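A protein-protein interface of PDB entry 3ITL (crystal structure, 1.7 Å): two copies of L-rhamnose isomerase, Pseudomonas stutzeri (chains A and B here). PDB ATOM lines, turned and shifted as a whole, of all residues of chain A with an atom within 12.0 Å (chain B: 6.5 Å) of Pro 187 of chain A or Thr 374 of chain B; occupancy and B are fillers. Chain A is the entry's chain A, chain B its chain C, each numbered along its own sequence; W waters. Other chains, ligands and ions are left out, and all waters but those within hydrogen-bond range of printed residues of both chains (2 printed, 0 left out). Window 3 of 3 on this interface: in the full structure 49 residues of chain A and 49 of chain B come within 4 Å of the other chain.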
ATOM      1  N   TYR A 143      -5.829   1.652  10.304  1.00  0.00           N
ATOM      2  CA  TYR A 143      -5.153   1.384  11.571  1.00  0.00           C
ATOM      3  C   TYR A 143      -5.225   2.540  12.562  1.00  0.00           C
ATOM      4  O   TYR A 143      -4.433   2.623  13.503  1.00  0.00           O
ATOM      5  CB  TYR A 143      -3.693   1.019  11.305  1.00  0.00           C
ATOM      6  CG  TYR A 143      -3.545  -0.193  10.418  1.00  0.00           C
ATOM      7  CD1 TYR A 143      -3.989  -1.447  10.840  1.00  0.00           C
ATOM      8  CD2 TYR A 143      -2.982  -0.087   9.147  1.00  0.00           C
ATOM      9  CE1 TYR A 143      -3.878  -2.564  10.017  1.00  0.00           C
ATOM     10  CE2 TYR A 143      -2.865  -1.201   8.317  1.00  0.00           C
ATOM     11  CZ  TYR A 143      -3.316  -2.436   8.759  1.00  0.00           C
ATOM     12  OH  TYR A 143      -3.208  -3.543   7.945  1.00  0.00           O
ATOM     13  N   GLY A 183      -8.250   1.907  17.869  1.00  0.00           N
ATOM     14  CA  GLY A 183      -8.065   0.873  18.866  1.00  0.00           C
ATOM     15  C   GLY A 183      -7.335  -0.293  18.238  1.00  0.00           C
ATOM     16  O   GLY A 183      -6.706  -0.147  17.184  1.00  0.00           O
ATOM     17  N   SER A 184      -7.416  -1.455  18.878  1.00  0.00           N
ATOM     18  CA  SER A 184      -6.755  -2.644  18.362  1.00  0.00           C
ATOM     19  C   SER A 184      -7.700  -3.826  18.459  1.00  0.00           C
ATOM     20  O   SER A 184      -8.635  -3.816  19.258  1.00  0.00           O
ATOM     21  CB  SER A 184      -5.492  -2.941  19.172  1.00  0.00           C
ATOM     22  OG  SER A 184      -5.801  -3.094  20.550  1.00  0.00           O
ATOM     23  N   ASN A 185      -7.458  -4.840  17.636  1.00  0.00           N
ATOM     24  CA  ASN A 185      -8.279  -6.041  17.655  1.00  0.00           C
ATOM     25  C   ASN A 185      -7.479  -7.202  18.228  1.00  0.00           C
ATOM     26  O   ASN A 185      -8.021  -8.281  18.441  1.00  0.00           O
ATOM     27  CB  ASN A 185      -8.753  -6.388  16.245  1.00  0.00           C
ATOM     28  CG  ASN A 185      -9.894  -5.504  15.782  1.00  0.00           C
ATOM     29  OD1 ASN A 185     -10.268  -4.553  16.467  1.00  0.00           O
ATOM     30  ND2 ASN A 185     -10.453  -5.814  14.615  1.00  0.00           N
ATOM     31  N   PHE A 186      -6.194  -6.966  18.486  1.00  0.00           N
ATOM     32  CA  PHE A 186      -5.320  -8.009  19.023  1.00  0.00           C
ATOM     33  C   PHE A 186      -4.399  -7.531  20.135  1.00  0.00           C
ATOM     34  O   PHE A 186      -3.892  -6.407  20.093  1.00  0.00           O
ATOM     35  CB  PHE A 186      -4.439  -8.577  17.910  1.00  0.00           C
ATOM     36  CG  PHE A 186      -5.204  -9.210  16.788  1.00  0.00           C
ATOM     37  CD1 PHE A 186      -5.602 -10.540  16.864  1.00  0.00           C
ATOM     38  CD2 PHE A 186      -5.525  -8.475  15.651  1.00  0.00           C
ATOM     39  CE1 PHE A 186      -6.309 -11.132  15.820  1.00  0.00           C
ATOM     40  CE2 PHE A 186      -6.230  -9.057  14.604  1.00  0.00           C
ATOM     41  CZ  PHE A 186      -6.622 -10.390  14.687  1.00  0.00           C
ATOM     42  N   PRO A 187      -4.178  -8.375  21.156  1.00  0.00           N
ATOM     43  CA  PRO A 187      -3.284  -7.972  22.242  1.00  0.00           C
ATOM     44  C   PRO A 187      -1.908  -7.724  21.617  1.00  0.00           C
ATOM     45  O   PRO A 187      -1.467  -8.488  20.752  1.00  0.00           O
ATOM     46  CB  PRO A 187      -3.285  -9.189  23.160  1.00  0.00           C
ATOM     47  CG  PRO A 187      -4.680  -9.717  23.005  1.00  0.00           C
ATOM     48  CD  PRO A 187      -4.915  -9.607  21.507  1.00  0.00           C
ATOM     49  N   GLY A 188      -1.244  -6.654  22.032  1.00  0.00           N
ATOM     50  CA  GLY A 188       0.070  -6.358  21.491  1.00  0.00           C
ATOM     51  C   GLY A 188       0.068  -5.481  20.253  1.00  0.00           C
ATOM     52  O   GLY A 188       1.056  -4.795  19.984  1.00  0.00           O
ATOM     53  N   GLN A 189      -1.025  -5.500  19.493  1.00  0.00           N
ATOM     54  CA  GLN A 189      -1.115  -4.688  18.281  1.00  0.00           C
ATOM     55  C   GLN A 189      -0.794  -3.222  18.561  1.00  0.00           C
ATOM     56  O   GLN A 189      -0.085  -2.576  17.785  1.00  0.00           O
ATOM     57  CB  GLN A 189      -2.514  -4.799  17.658  1.00  0.00           C
ATOM     58  CG  GLN A 189      -2.738  -3.828  16.502  1.00  0.00           C
ATOM     59  CD  GLN A 189      -4.129  -3.910  15.898  1.00  0.00           C
ATOM     60  OE1 GLN A 189      -4.468  -3.138  14.995  1.00  0.00           O
ATOM     61  NE2 GLN A 189      -4.936  -4.841  16.384  1.00  0.00           N
ATOM     62  N   SER A 190      -1.314  -2.703  19.671  1.00  0.00           N
ATOM     63  CA  SER A 190      -1.087  -1.311  20.051  1.00  0.00           C
ATOM     64  C   SER A 190      -0.407  -1.178  21.406  1.00  0.00           C
ATOM     65  O   SER A 190      -0.568  -2.025  22.283  1.00  0.00           O
ATOM     66  CB  SER A 190      -2.419  -0.543  20.134  1.00  0.00           C
ATOM     67  OG  SER A 190      -3.125  -0.525  18.905  1.00  0.00           O
ATOM     68  N   ASN A 191       0.367  -0.112  21.565  1.00  0.00           N
ATOM     69  CA  ASN A 191       0.989   0.184  22.845  1.00  0.00           C
ATOM     70  C   ASN A 191      -0.061   1.143  23.407  1.00  0.00           C
ATOM     71  O   ASN A 191      -0.211   2.258  22.910  1.00  0.00           O
ATOM     72  CB  ASN A 191       2.326   0.904  22.656  1.00  0.00           C
ATOM     73  CG  ASN A 191       2.930   1.359  23.972  1.00  0.00           C
ATOM     74  OD1 ASN A 191       2.319   2.124  24.718  1.00  0.00           O
ATOM     75  ND2 ASN A 191       4.136   0.885  24.265  1.00  0.00           N
ATOM     76  N   PHE A 192      -0.805   0.697  24.415  1.00  0.00           N
ATOM     77  CA  PHE A 192      -1.876   1.504  25.002  1.00  0.00           C
ATOM     78  C   PHE A 192      -1.514   2.951  25.295  1.00  0.00           C
ATOM     79  O   PHE A 192      -2.227   3.876  24.899  1.00  0.00           O
ATOM     80  CB  PHE A 192      -2.386   0.871  26.303  1.00  0.00           C
ATOM     81  CG  PHE A 192      -2.971  -0.508  26.136  1.00  0.00           C
ATOM     82  CD1 PHE A 192      -3.722  -0.839  25.012  1.00  0.00           C
ATOM     83  CD2 PHE A 192      -2.812  -1.460  27.139  1.00  0.00           C
ATOM     84  CE1 PHE A 192      -4.306  -2.104  24.891  1.00  0.00           C
ATOM     85  CE2 PHE A 192      -3.393  -2.724  27.029  1.00  0.00           C
ATOM     86  CZ  PHE A 192      -4.140  -3.045  25.904  1.00  0.00           C
ATOM     87  N   THR A 193      -0.410   3.146  26.003  1.00  0.00           N
ATOM     88  CA  THR A 193       0.018   4.485  26.373  1.00  0.00           C
ATOM     89  C   THR A 193       0.475   5.351  25.207  1.00  0.00           C
ATOM     90  O   THR A 193       0.082   6.511  25.110  1.00  0.00           O
ATOM     91  CB  THR A 193       1.119   4.410  27.444  1.00  0.00           C
ATOM     92  OG1 THR A 193       0.571   3.807  28.624  1.00  0.00           O
ATOM     93  CG2 THR A 193       1.644   5.802  27.783  1.00  0.00           C
ATOM     94  N   ALA A 195      -0.360   5.099  22.065  1.00  0.00           N
ATOM     95  CA  ALA A 195      -1.507   5.416  21.221  1.00  0.00           C
ATOM     96  C   ALA A 195      -2.296   6.569  21.843  1.00  0.00           C
ATOM     97  O   ALA A 195      -2.724   7.480  21.142  1.00  0.00           O
ATOM     98  CB  ALA A 195      -2.404   4.193  21.064  1.00  0.00           C
ATOM     99  N   ALA A 226     -13.282  -1.388  17.190  1.00  0.00           N
ATOM    100  CA  ALA A 226     -12.138  -2.119  17.748  1.00  0.00           C
ATOM    101  C   ALA A 226     -12.662  -3.163  18.730  1.00  0.00           C
ATOM    102  O   ALA A 226     -13.448  -2.843  19.624  1.00  0.00           O
ATOM    103  CB  ALA A 226     -11.181  -1.161  18.446  1.00  0.00           C
ATOM    104  N   PHE A 227     -12.212  -4.407  18.578  1.00  0.00           N
ATOM    105  CA  PHE A 227     -12.705  -5.480  19.425  1.00  0.00           C
ATOM    106  C   PHE A 227     -11.791  -6.051  20.509  1.00  0.00           C
ATOM    107  O   PHE A 227     -12.098  -7.088  21.096  1.00  0.00           O
ATOM    108  CB  PHE A 227     -13.265  -6.592  18.532  1.00  0.00           C
ATOM    109  CG  PHE A 227     -14.387  -6.120  17.639  1.00  0.00           C
ATOM    110  CD1 PHE A 227     -15.554  -5.606  18.194  1.00  0.00           C
ATOM    111  CD2 PHE A 227     -14.258  -6.143  16.254  1.00  0.00           C
ATOM    112  CE1 PHE A 227     -16.579  -5.119  17.386  1.00  0.00           C
ATOM    113  CE2 PHE A 227     -15.279  -5.656  15.435  1.00  0.00           C
ATOM    114  CZ  PHE A 227     -16.441  -5.142  16.006  1.00  0.00           C
ATOM    115  N   TYR A 228     -10.667  -5.387  20.768  1.00  0.00           N
ATOM    116  CA  TYR A 228      -9.793  -5.804  21.858  1.00  0.00           C
ATOM    117  C   TYR A 228      -9.593  -4.586  22.770  1.00  0.00           C
ATOM    118  O   TYR A 228      -9.884  -4.644  23.965  1.00  0.00           O
ATOM    119  CB  TYR A 228      -8.437  -6.325  21.374  1.00  0.00           C
ATOM    120  CG  TYR A 228      -7.485  -6.491  22.536  1.00  0.00           C
ATOM    121  CD1 TYR A 228      -7.796  -7.344  23.597  1.00  0.00           C
ATOM    122  CD2 TYR A 228      -6.343  -5.703  22.641  1.00  0.00           C
ATOM    123  CE1 TYR A 228      -7.002  -7.392  24.734  1.00  0.00           C
ATOM    124  CE2 TYR A 228      -5.541  -5.744  23.770  1.00  0.00           C
ATOM    125  CZ  TYR A 228      -5.877  -6.584  24.815  1.00  0.00           C
ATOM    126  OH  TYR A 228      -5.107  -6.582  25.952  1.00  0.00           O
ATOM    127  N   SER A 229      -9.098  -3.485  22.209  1.00  0.00           N
ATOM    128  CA  SER A 229      -8.919  -2.260  22.985  1.00  0.00           C
ATOM    129  C   SER A 229      -9.352  -1.068  22.138  1.00  0.00           C
ATOM    130  O   SER A 229      -9.328  -1.121  20.910  1.00  0.00           O
ATOM    131  CB  SER A 229      -7.454  -2.075  23.423  1.00  0.00           C
ATOM    132  OG  SER A 229      -6.665  -1.452  22.416  1.00  0.00           O
ATOM    133  N   THR A 230      -9.772  -0.001  22.807  1.00  0.00           N
ATOM    134  CA  THR A 230     -10.194   1.221  22.135  1.00  0.00           C
ATOM    135  C   THR A 230      -9.468   2.336  22.878  1.00  0.00           C
ATOM    136  O   THR A 230      -9.400   2.313  24.107  1.00  0.00           O
ATOM    137  CB  THR A 230     -11.729   1.398  22.229  1.00  0.00           C
ATOM    138  OG1 THR A 230     -12.364   0.435  21.377  1.00  0.00           O
ATOM    139  CG2 THR A 230     -12.146   2.810  21.809  1.00  0.00           C
ATOM    140  N   GLU B 265      -6.135  -4.655  31.536  1.00  0.00           N
ATOM    141  CA  GLU B 265      -4.750  -4.291  31.267  1.00  0.00           C
ATOM    142  C   GLU B 265      -4.631  -2.847  30.758  1.00  0.00           C
ATOM    143  O   GLU B 265      -3.600  -2.203  30.953  1.00  0.00           O
ATOM    144  CB  GLU B 265      -4.098  -5.286  30.284  1.00  0.00           C
ATOM    145  CG  GLU B 265      -4.897  -5.589  29.019  1.00  0.00           C
ATOM    146  CD  GLU B 265      -5.839  -6.778  29.166  1.00  0.00           C
ATOM    147  OE1 GLU B 265      -6.328  -7.028  30.285  1.00  0.00           O
ATOM    148  OE2 GLU B 265      -6.105  -7.459  28.152  1.00  0.00           O
ATOM    149  N   TYR B 300      -4.177 -16.059  30.331  1.00  0.00           N
ATOM    150  CA  TYR B 300      -3.653 -15.106  29.354  1.00  0.00           C
ATOM    151  C   TYR B 300      -3.872 -13.672  29.815  1.00  0.00           C
ATOM    152  O   TYR B 300      -3.005 -12.817  29.632  1.00  0.00           O
ATOM    153  CB  TYR B 300      -4.289 -15.330  27.973  1.00  0.00           C
ATOM    154  CG  TYR B 300      -3.536 -14.659  26.841  1.00  0.00           C
ATOM    155  CD1 TYR B 300      -2.139 -14.693  26.789  1.00  0.00           C
ATOM    156  CD2 TYR B 300      -4.214 -14.001  25.814  1.00  0.00           C
ATOM    157  CE1 TYR B 300      -1.438 -14.087  25.745  1.00  0.00           C
ATOM    158  CE2 TYR B 300      -3.519 -13.393  24.763  1.00  0.00           C
ATOM    159  CZ  TYR B 300      -2.132 -13.440  24.739  1.00  0.00           C
ATOM    160  OH  TYR B 300      -1.431 -12.837  23.712  1.00  0.00           O
ATOM    161  N   LEU B 304      -1.256 -10.709  30.192  1.00  0.00           N
ATOM    162  CA  LEU B 304      -1.398  -9.401  29.560  1.00  0.00           C
ATOM    163  C   LEU B 304      -1.245  -8.245  30.546  1.00  0.00           C
ATOM    164  O   LEU B 304      -0.734  -7.179  30.187  1.00  0.00           O
ATOM    165  CB  LEU B 304      -2.734  -9.319  28.806  1.00  0.00           C
ATOM    166  CG  LEU B 304      -2.816 -10.286  27.614  1.00  0.00           C
ATOM    167  CD1 LEU B 304      -4.169 -10.169  26.931  1.00  0.00           C
ATOM    168  CD2 LEU B 304      -1.688  -9.982  26.627  1.00  0.00           C
ATOM    169  N   ASN B 307       2.304  -7.982  31.114  1.00  0.00           N
ATOM    170  CA  ASN B 307       2.979  -7.464  29.935  1.00  0.00           C
ATOM    171  C   ASN B 307       3.077  -5.939  30.051  1.00  0.00           C
ATOM    172  O   ASN B 307       4.079  -5.340  29.656  1.00  0.00           O
ATOM    173  CB  ASN B 307       2.216  -7.859  28.666  1.00  0.00           C
ATOM    174  CG  ASN B 307       2.818  -7.256  27.409  1.00  0.00           C
ATOM    175  OD1 ASN B 307       4.007  -7.423  27.131  1.00  0.00           O
ATOM    176  ND2 ASN B 307       1.994  -6.552  26.639  1.00  0.00           N
ATOM    177  N   LEU B 361       8.427  -6.402  19.211  1.00  0.00           N
ATOM    178  CA  LEU B 361       7.064  -5.941  19.455  1.00  0.00           C
ATOM    179  C   LEU B 361       6.892  -4.489  19.029  1.00  0.00           C
ATOM    180  O   LEU B 361       5.939  -4.147  18.329  1.00  0.00           O
ATOM    181  CB  LEU B 361       6.704  -6.096  20.938  1.00  0.00           C
ATOM    182  CG  LEU B 361       5.279  -5.687  21.326  1.00  0.00           C
ATOM    183  CD1 LEU B 361       4.265  -6.481  20.503  1.00  0.00           C
ATOM    184  CD2 LEU B 361       5.066  -5.929  22.810  1.00  0.00           C
ATOM    185  N   TYR B 364       6.677  -4.155  15.242  1.00  0.00           N
ATOM    186  CA  TYR B 364       5.400  -4.577  14.680  1.00  0.00           C
ATOM    187  C   TYR B 364       4.288  -3.598  15.031  1.00  0.00           C
ATOM    188  O   TYR B 364       3.309  -3.480  14.300  1.00  0.00           O
ATOM    189  CB  TYR B 364       5.033  -5.982  15.167  1.00  0.00           C
ATOM    190  CG  TYR B 364       5.956  -7.060  14.638  1.00  0.00           C
ATOM    191  CD1 TYR B 364       6.238  -7.158  13.274  1.00  0.00           C
ATOM    192  CD2 TYR B 364       6.537  -7.988  15.498  1.00  0.00           C
ATOM    193  CE1 TYR B 364       7.080  -8.161  12.781  1.00  0.00           C
ATOM    194  CE2 TYR B 364       7.377  -8.990  15.018  1.00  0.00           C
ATOM    195  CZ  TYR B 364       7.644  -9.071  13.664  1.00  0.00           C
ATOM    196  OH  TYR B 364       8.470 -10.068  13.196  1.00  0.00           O
ATOM    197  N   ASP B 369       1.632  -4.139  12.205  1.00  0.00           N
ATOM    198  CA  ASP B 369       1.603  -5.557  11.866  1.00  0.00           C
ATOM    199  C   ASP B 369       0.931  -6.247  13.048  1.00  0.00           C
ATOM    200  O   ASP B 369       1.598  -6.856  13.888  1.00  0.00           O
ATOM    201  CB  ASP B 369       3.027  -6.087  11.697  1.00  0.00           C
ATOM    202  CG  ASP B 369       3.071  -7.453  11.038  1.00  0.00           C
ATOM    203  OD1 ASP B 369       2.042  -8.164  11.046  1.00  0.00           O
ATOM    204  OD2 ASP B 369       4.149  -7.819  10.521  1.00  0.00           O
ATOM    205  N   ALA B 370      -0.393  -6.136  13.114  1.00  0.00           N
ATOM    206  CA  ALA B 370      -1.168  -6.713  14.206  1.00  0.00           C
ATOM    207  C   ALA B 370      -0.920  -8.199  14.434  1.00  0.00           C
ATOM    208  O   ALA B 370      -0.733  -8.638  15.570  1.00  0.00           O
ATOM    209  CB  ALA B 370      -2.657  -6.466  13.965  1.00  0.00           C
ATOM    210  N   LEU B 371      -0.929  -8.974  13.357  1.00  0.00           N
ATOM    211  CA  LEU B 371      -0.720 -10.410  13.461  1.00  0.00           C
ATOM    212  C   LEU B 371       0.620 -10.768  14.099  1.00  0.00           C
ATOM    213  O   LEU B 371       0.669 -11.582  15.019  1.00  0.00           O
ATOM    214  CB  LEU B 371      -0.830 -11.065  12.085  1.00  0.00           C
ATOM    215  CG  LEU B 371      -0.661 -12.590  12.105  1.00  0.00           C
ATOM    216  CD1 LEU B 371      -1.894 -13.271  11.525  1.00  0.00           C
ATOM    217  CD2 LEU B 371       0.588 -12.967  11.319  1.00  0.00           C
ATOM    218  N   MET B 372       1.707 -10.168  13.622  1.00  0.00           N
ATOM    219  CA  MET B 372       3.014 -10.473  14.197  1.00  0.00           C
ATOM    220  C   MET B 372       3.179  -9.878  15.590  1.00  0.00           C
ATOM    221  O   MET B 372       3.923 -10.411  16.411  1.00  0.00           O
ATOM    222  CB  MET B 372       4.143  -9.988  13.284  1.00  0.00           C
ATOM    223  CG  MET B 372       4.406 -10.897  12.087  1.00  0.00           C
ATOM    224  SD  MET B 372       4.587 -12.652  12.533  1.00  0.00           S
ATOM    225  CE  MET B 372       5.902 -12.582  13.749  1.00  0.00           C
ATOM    226  N   ALA B 373       2.493  -8.771  15.859  1.00  0.00           N
ATOM    227  CA  ALA B 373       2.566  -8.144  17.172  1.00  0.00           C
ATOM    228  C   ALA B 373       1.953  -9.094  18.199  1.00  0.00           C
ATOM    229  O   ALA B 373       2.534  -9.351  19.255  1.00  0.00           O
ATOM    230  CB  ALA B 373       1.805  -6.819  17.168  1.00  0.00           C
ATOM    231  N   THR B 374       0.777  -9.624  17.881  1.00  0.00           N
ATOM    232  CA  THR B 374       0.106 -10.538  18.794  1.00  0.00           C
ATOM    233  C   THR B 374       0.882 -11.855  18.900  1.00  0.00           C
ATOM    234  O   THR B 374       0.967 -12.449  19.974  1.00  0.00           O
ATOM    235  CB  THR B 374      -1.360 -10.782  18.343  1.00  0.00           C
ATOM    236  OG1 THR B 374      -2.200 -10.872  19.499  1.00  0.00           O
ATOM    237  CG2 THR B 374      -1.484 -12.064  17.518  1.00  0.00           C
ATOM    238  N   GLU B 375       1.464 -12.305  17.794  1.00  0.00           N
ATOM    239  CA  GLU B 375       2.242 -13.542  17.809  1.00  0.00           C
ATOM    240  C   GLU B 375       3.512 -13.346  18.635  1.00  0.00           C
ATOM    241  O   GLU B 375       4.030 -14.295  19.226  1.00  0.00           O
ATOM    242  CB  GLU B 375       2.590 -13.967  16.377  1.00  0.00           C
ATOM    243  CG  GLU B 375       3.635 -15.085  16.241  1.00  0.00           C
ATOM    244  CD  GLU B 375       3.212 -16.421  16.846  1.00  0.00           C
ATOM    245  OE1 GLU B 375       2.027 -16.584  17.218  1.00  0.00           O
ATOM    246  OE2 GLU B 375       4.080 -17.320  16.935  1.00  0.00           O
ATOM    247  N   THR B 376       4.012 -12.113  18.684  1.00  0.00           N
ATOM    248  CA  THR B 376       5.213 -11.829  19.462  1.00  0.00           C
ATOM    249  C   THR B 376       4.910 -12.042  20.943  1.00  0.00           C
ATOM    250  O   THR B 376       5.753 -12.539  21.692  1.00  0.00           O
ATOM    251  CB  THR B 376       5.717 -10.384  19.221  1.00  0.00           C
ATOM    252  OG1 THR B 376       6.140 -10.253  17.858  1.00  0.00           O
ATOM    253  CG2 THR B 376       6.895 -10.063  20.132  1.00  0.00           C
ATOM    254  N   LEU B 377       3.701 -11.672  21.362  1.00  0.00           N
ATOM    255  CA  LEU B 377       3.305 -11.867  22.754  1.00  0.00           C
ATOM    256  C   LEU B 377       3.092 -13.356  23.007  1.00  0.00           C
ATOM    257  O   LEU B 377       3.530 -13.887  24.026  1.00  0.00           O
ATOM    258  CB  LEU B 377       2.007 -11.112  23.071  1.00  0.00           C
ATOM    259  CG  LEU B 377       2.032  -9.581  23.104  1.00  0.00           C
ATOM    260  CD1 LEU B 377       0.686  -9.076  23.609  1.00  0.00           C
ATOM    261  CD2 LEU B 377       3.147  -9.090  24.024  1.00  0.00           C
ATOM    262  N   LYS B 378       2.427 -14.028  22.070  1.00  0.00           N
ATOM    263  CA  LYS B 378       2.157 -15.457  22.210  1.00  0.00           C
ATOM    264  C   LYS B 378       3.424 -16.302  22.283  1.00  0.00           C
ATOM    265  O   LYS B 378       3.453 -17.314  22.980  1.00  0.00           O
ATOM    266  CB  LYS B 378       1.273 -15.956  21.064  1.00  0.00           C
ATOM    267  CG  LYS B 378      -0.204 -15.579  21.202  1.00  0.00           C
ATOM    268  CD  LYS B 378      -0.790 -16.127  22.496  1.00  0.00           C
ATOM    269  CE  LYS B 378      -2.315 -16.072  22.500  1.00  0.00           C
ATOM    270  NZ  LYS B 378      -2.908 -17.008  21.493  1.00  0.00           N
ATOM    271  N   ARG B 379       4.470 -15.899  21.570  1.00  0.00           N
ATOM    272  CA  ARG B 379       5.706 -16.667  21.614  1.00  0.00           C
ATOM    273  C   ARG B 379       6.250 -16.698  23.035  1.00  0.00           C
ATOM    274  O   ARG B 379       6.859 -17.681  23.454  1.00  0.00           O
ATOM    275  CB  ARG B 379       6.729 -16.080  20.640  1.00  0.00           C
ATOM    276  CG  ARG B 379       6.345 -16.372  19.206  1.00  0.00           C
ATOM    277  CD  ARG B 379       7.288 -15.771  18.185  1.00  0.00           C
ATOM    278  NE  ARG B 379       6.923 -16.228  16.847  1.00  0.00           N
ATOM    279  CZ  ARG B 379       7.533 -15.858  15.728  1.00  0.00           C
ATOM    280  NH1 ARG B 379       8.552 -15.011  15.771  1.00  0.00           N
ATOM    281  NH2 ARG B 379       7.124 -16.343  14.562  1.00  0.00           N
HETATM  282  O   HOH W   1      -1.933  -5.792  10.298  1.00  0.00           O
HETATM  283  O   HOH W   2       0.405  -3.570  15.106  1.00  0.00           O
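Of the 17 printed residues of chain B, 7 touch a printed residue of chain A.
Hydrophobic or aromatic side chains of chain B within 4 Å of the printed part of chain A: Leu 304, Leu 361, Ala 370, Ala 373 and Leu 377.
Of the 18 printed residues of chain A, 6 touch a printed residue of chain B.
Hydrophobic or aromatic side chains of chain A that line the printed part of chain B: Phe 186, Pro 187, Phe 192 and Tyr 228.
Along chain A the printed residues that touch a printed residue of chain B span positions 186 to 228.
Among the printed residues, 13 pairs touch across the chains.
Among the printed residues, no Asp or Glu carboxylate lies within 4 Å of a Lys or Arg side-chain nitrogen of the other chain.
The backbone carbonyl oxygen of Ser 184 of chain A is in hydrogen-bond range of the backbone NH of Tyr 228 of chain A (3.0 Å).
The backbone NH of Asn 185 of chain A lies close to the side-chain amide nitrogen of Gln 189 of chain A (2.8 Å).
The backbone NH of Phe 186 of chain A sits close to the side-chain amide nitrogen of Gln 189 of chain A, at 3.2 Å.
Water W2 lies within hydrogen-bond range of O of Gln 189 of chain A (2.9 Å), O of Tyr 364 of chain B (3.0 Å), N of Asp 369 of chain B (3.2 Å) and N of Ala 370 of chain B (3.3 Å).
Water W1 bridges the backbone NH of Ala 370 of chain B (3.2 Å) and the side-chain hydroxyl of Tyr 143 of chain A (3.5 Å).
The side-chain hydroxyl (OG1) of Thr 374 of chain B lies within hydrogen-bond range of the backbone carbonyl oxygen (O) of Pro 187 of chain A.
The side-chain carboxylate (OE2) of Glu 265 of chain B is in hydrogen-bond range of the side-chain hydroxyl (OH) of Tyr 228 of chain A, at 2.6 Å.
Thr 374 of chain B touches just these residues of chain A: Phe 186 and Pro 187.
Leu 304 of chain B touches two residues of chain A.
Of chain A, only Phe 186 (3.9 Å) and Gln 189 (3.5 Å) come within 4 Å of Ala 370 of chain B.
Of chain A, only Gly 188 and Gln 189 come within 4 Å of Ala 373 of chain B.
No residue of chain A comes within 4 Å of Glu 375 of chain B.
Leu 377 of chain B touches just these residues of chain A: Pro 187 (3.5 Å) and Gly 188 (3.5 Å).
No residue of chain A comes within 4 Å of Lys 378 of chain B.
Of the printed residues of chain B, Gly 188 of chain A touches Leu 361 (3.7 Å), Ala 373 (3.5 Å) and Leu 377 (3.5 Å).
Of the printed residues of chain B, Phe 186 of chain A touches Ala 370 (3.9 Å) and Thr 374 (3.6 Å).
The nearest residue of chain B that does not touch Pro 187 of chain A is Tyr 300 of chain B (4.1 Å).
The nearest residue of chain A that does not touch Thr 374 of chain B is Gln 189 of chain A (4.8 Å).
The nearest printed residue of chain A that does not touch Glu 265 of chain B is Pro 187 of chain A (5.8 Å).
No position is printed for both chains.
Of the 13 pairs that touch across the chains among the printed residues, none has its exchanged pair printed and touching as well.
Among the printed residues, merely in contact across the chains: Phe 186 of chain A with Ala 370 of chain B (3.9 Å), Phe 186 of chain A with Thr 374 of chain B (3.6 Å), Pro 187 of chain A with Leu 304 of chain B (3.9 Å), Pro 187 of chain A with Leu 377 of chain B (3.5 Å), Gly 188 of chain A with Leu 361 of chain B (3.7 Å), Gly 188 of chain A with Ala 373 of chain B (3.5 Å), Gly 188 of chain A with Leu 377 of chain B (3.5 Å), Gln 189 of chain A with Ala 370 of chain B (3.5 Å), Gln 189 of chain A with Ala 373 of chain B (3.8 Å), Phe 192 of chain A with Glu 265 of chain B (3.8 Å) and Tyr 228 of chain A with Leu 304 of chain B (3.8 Å).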
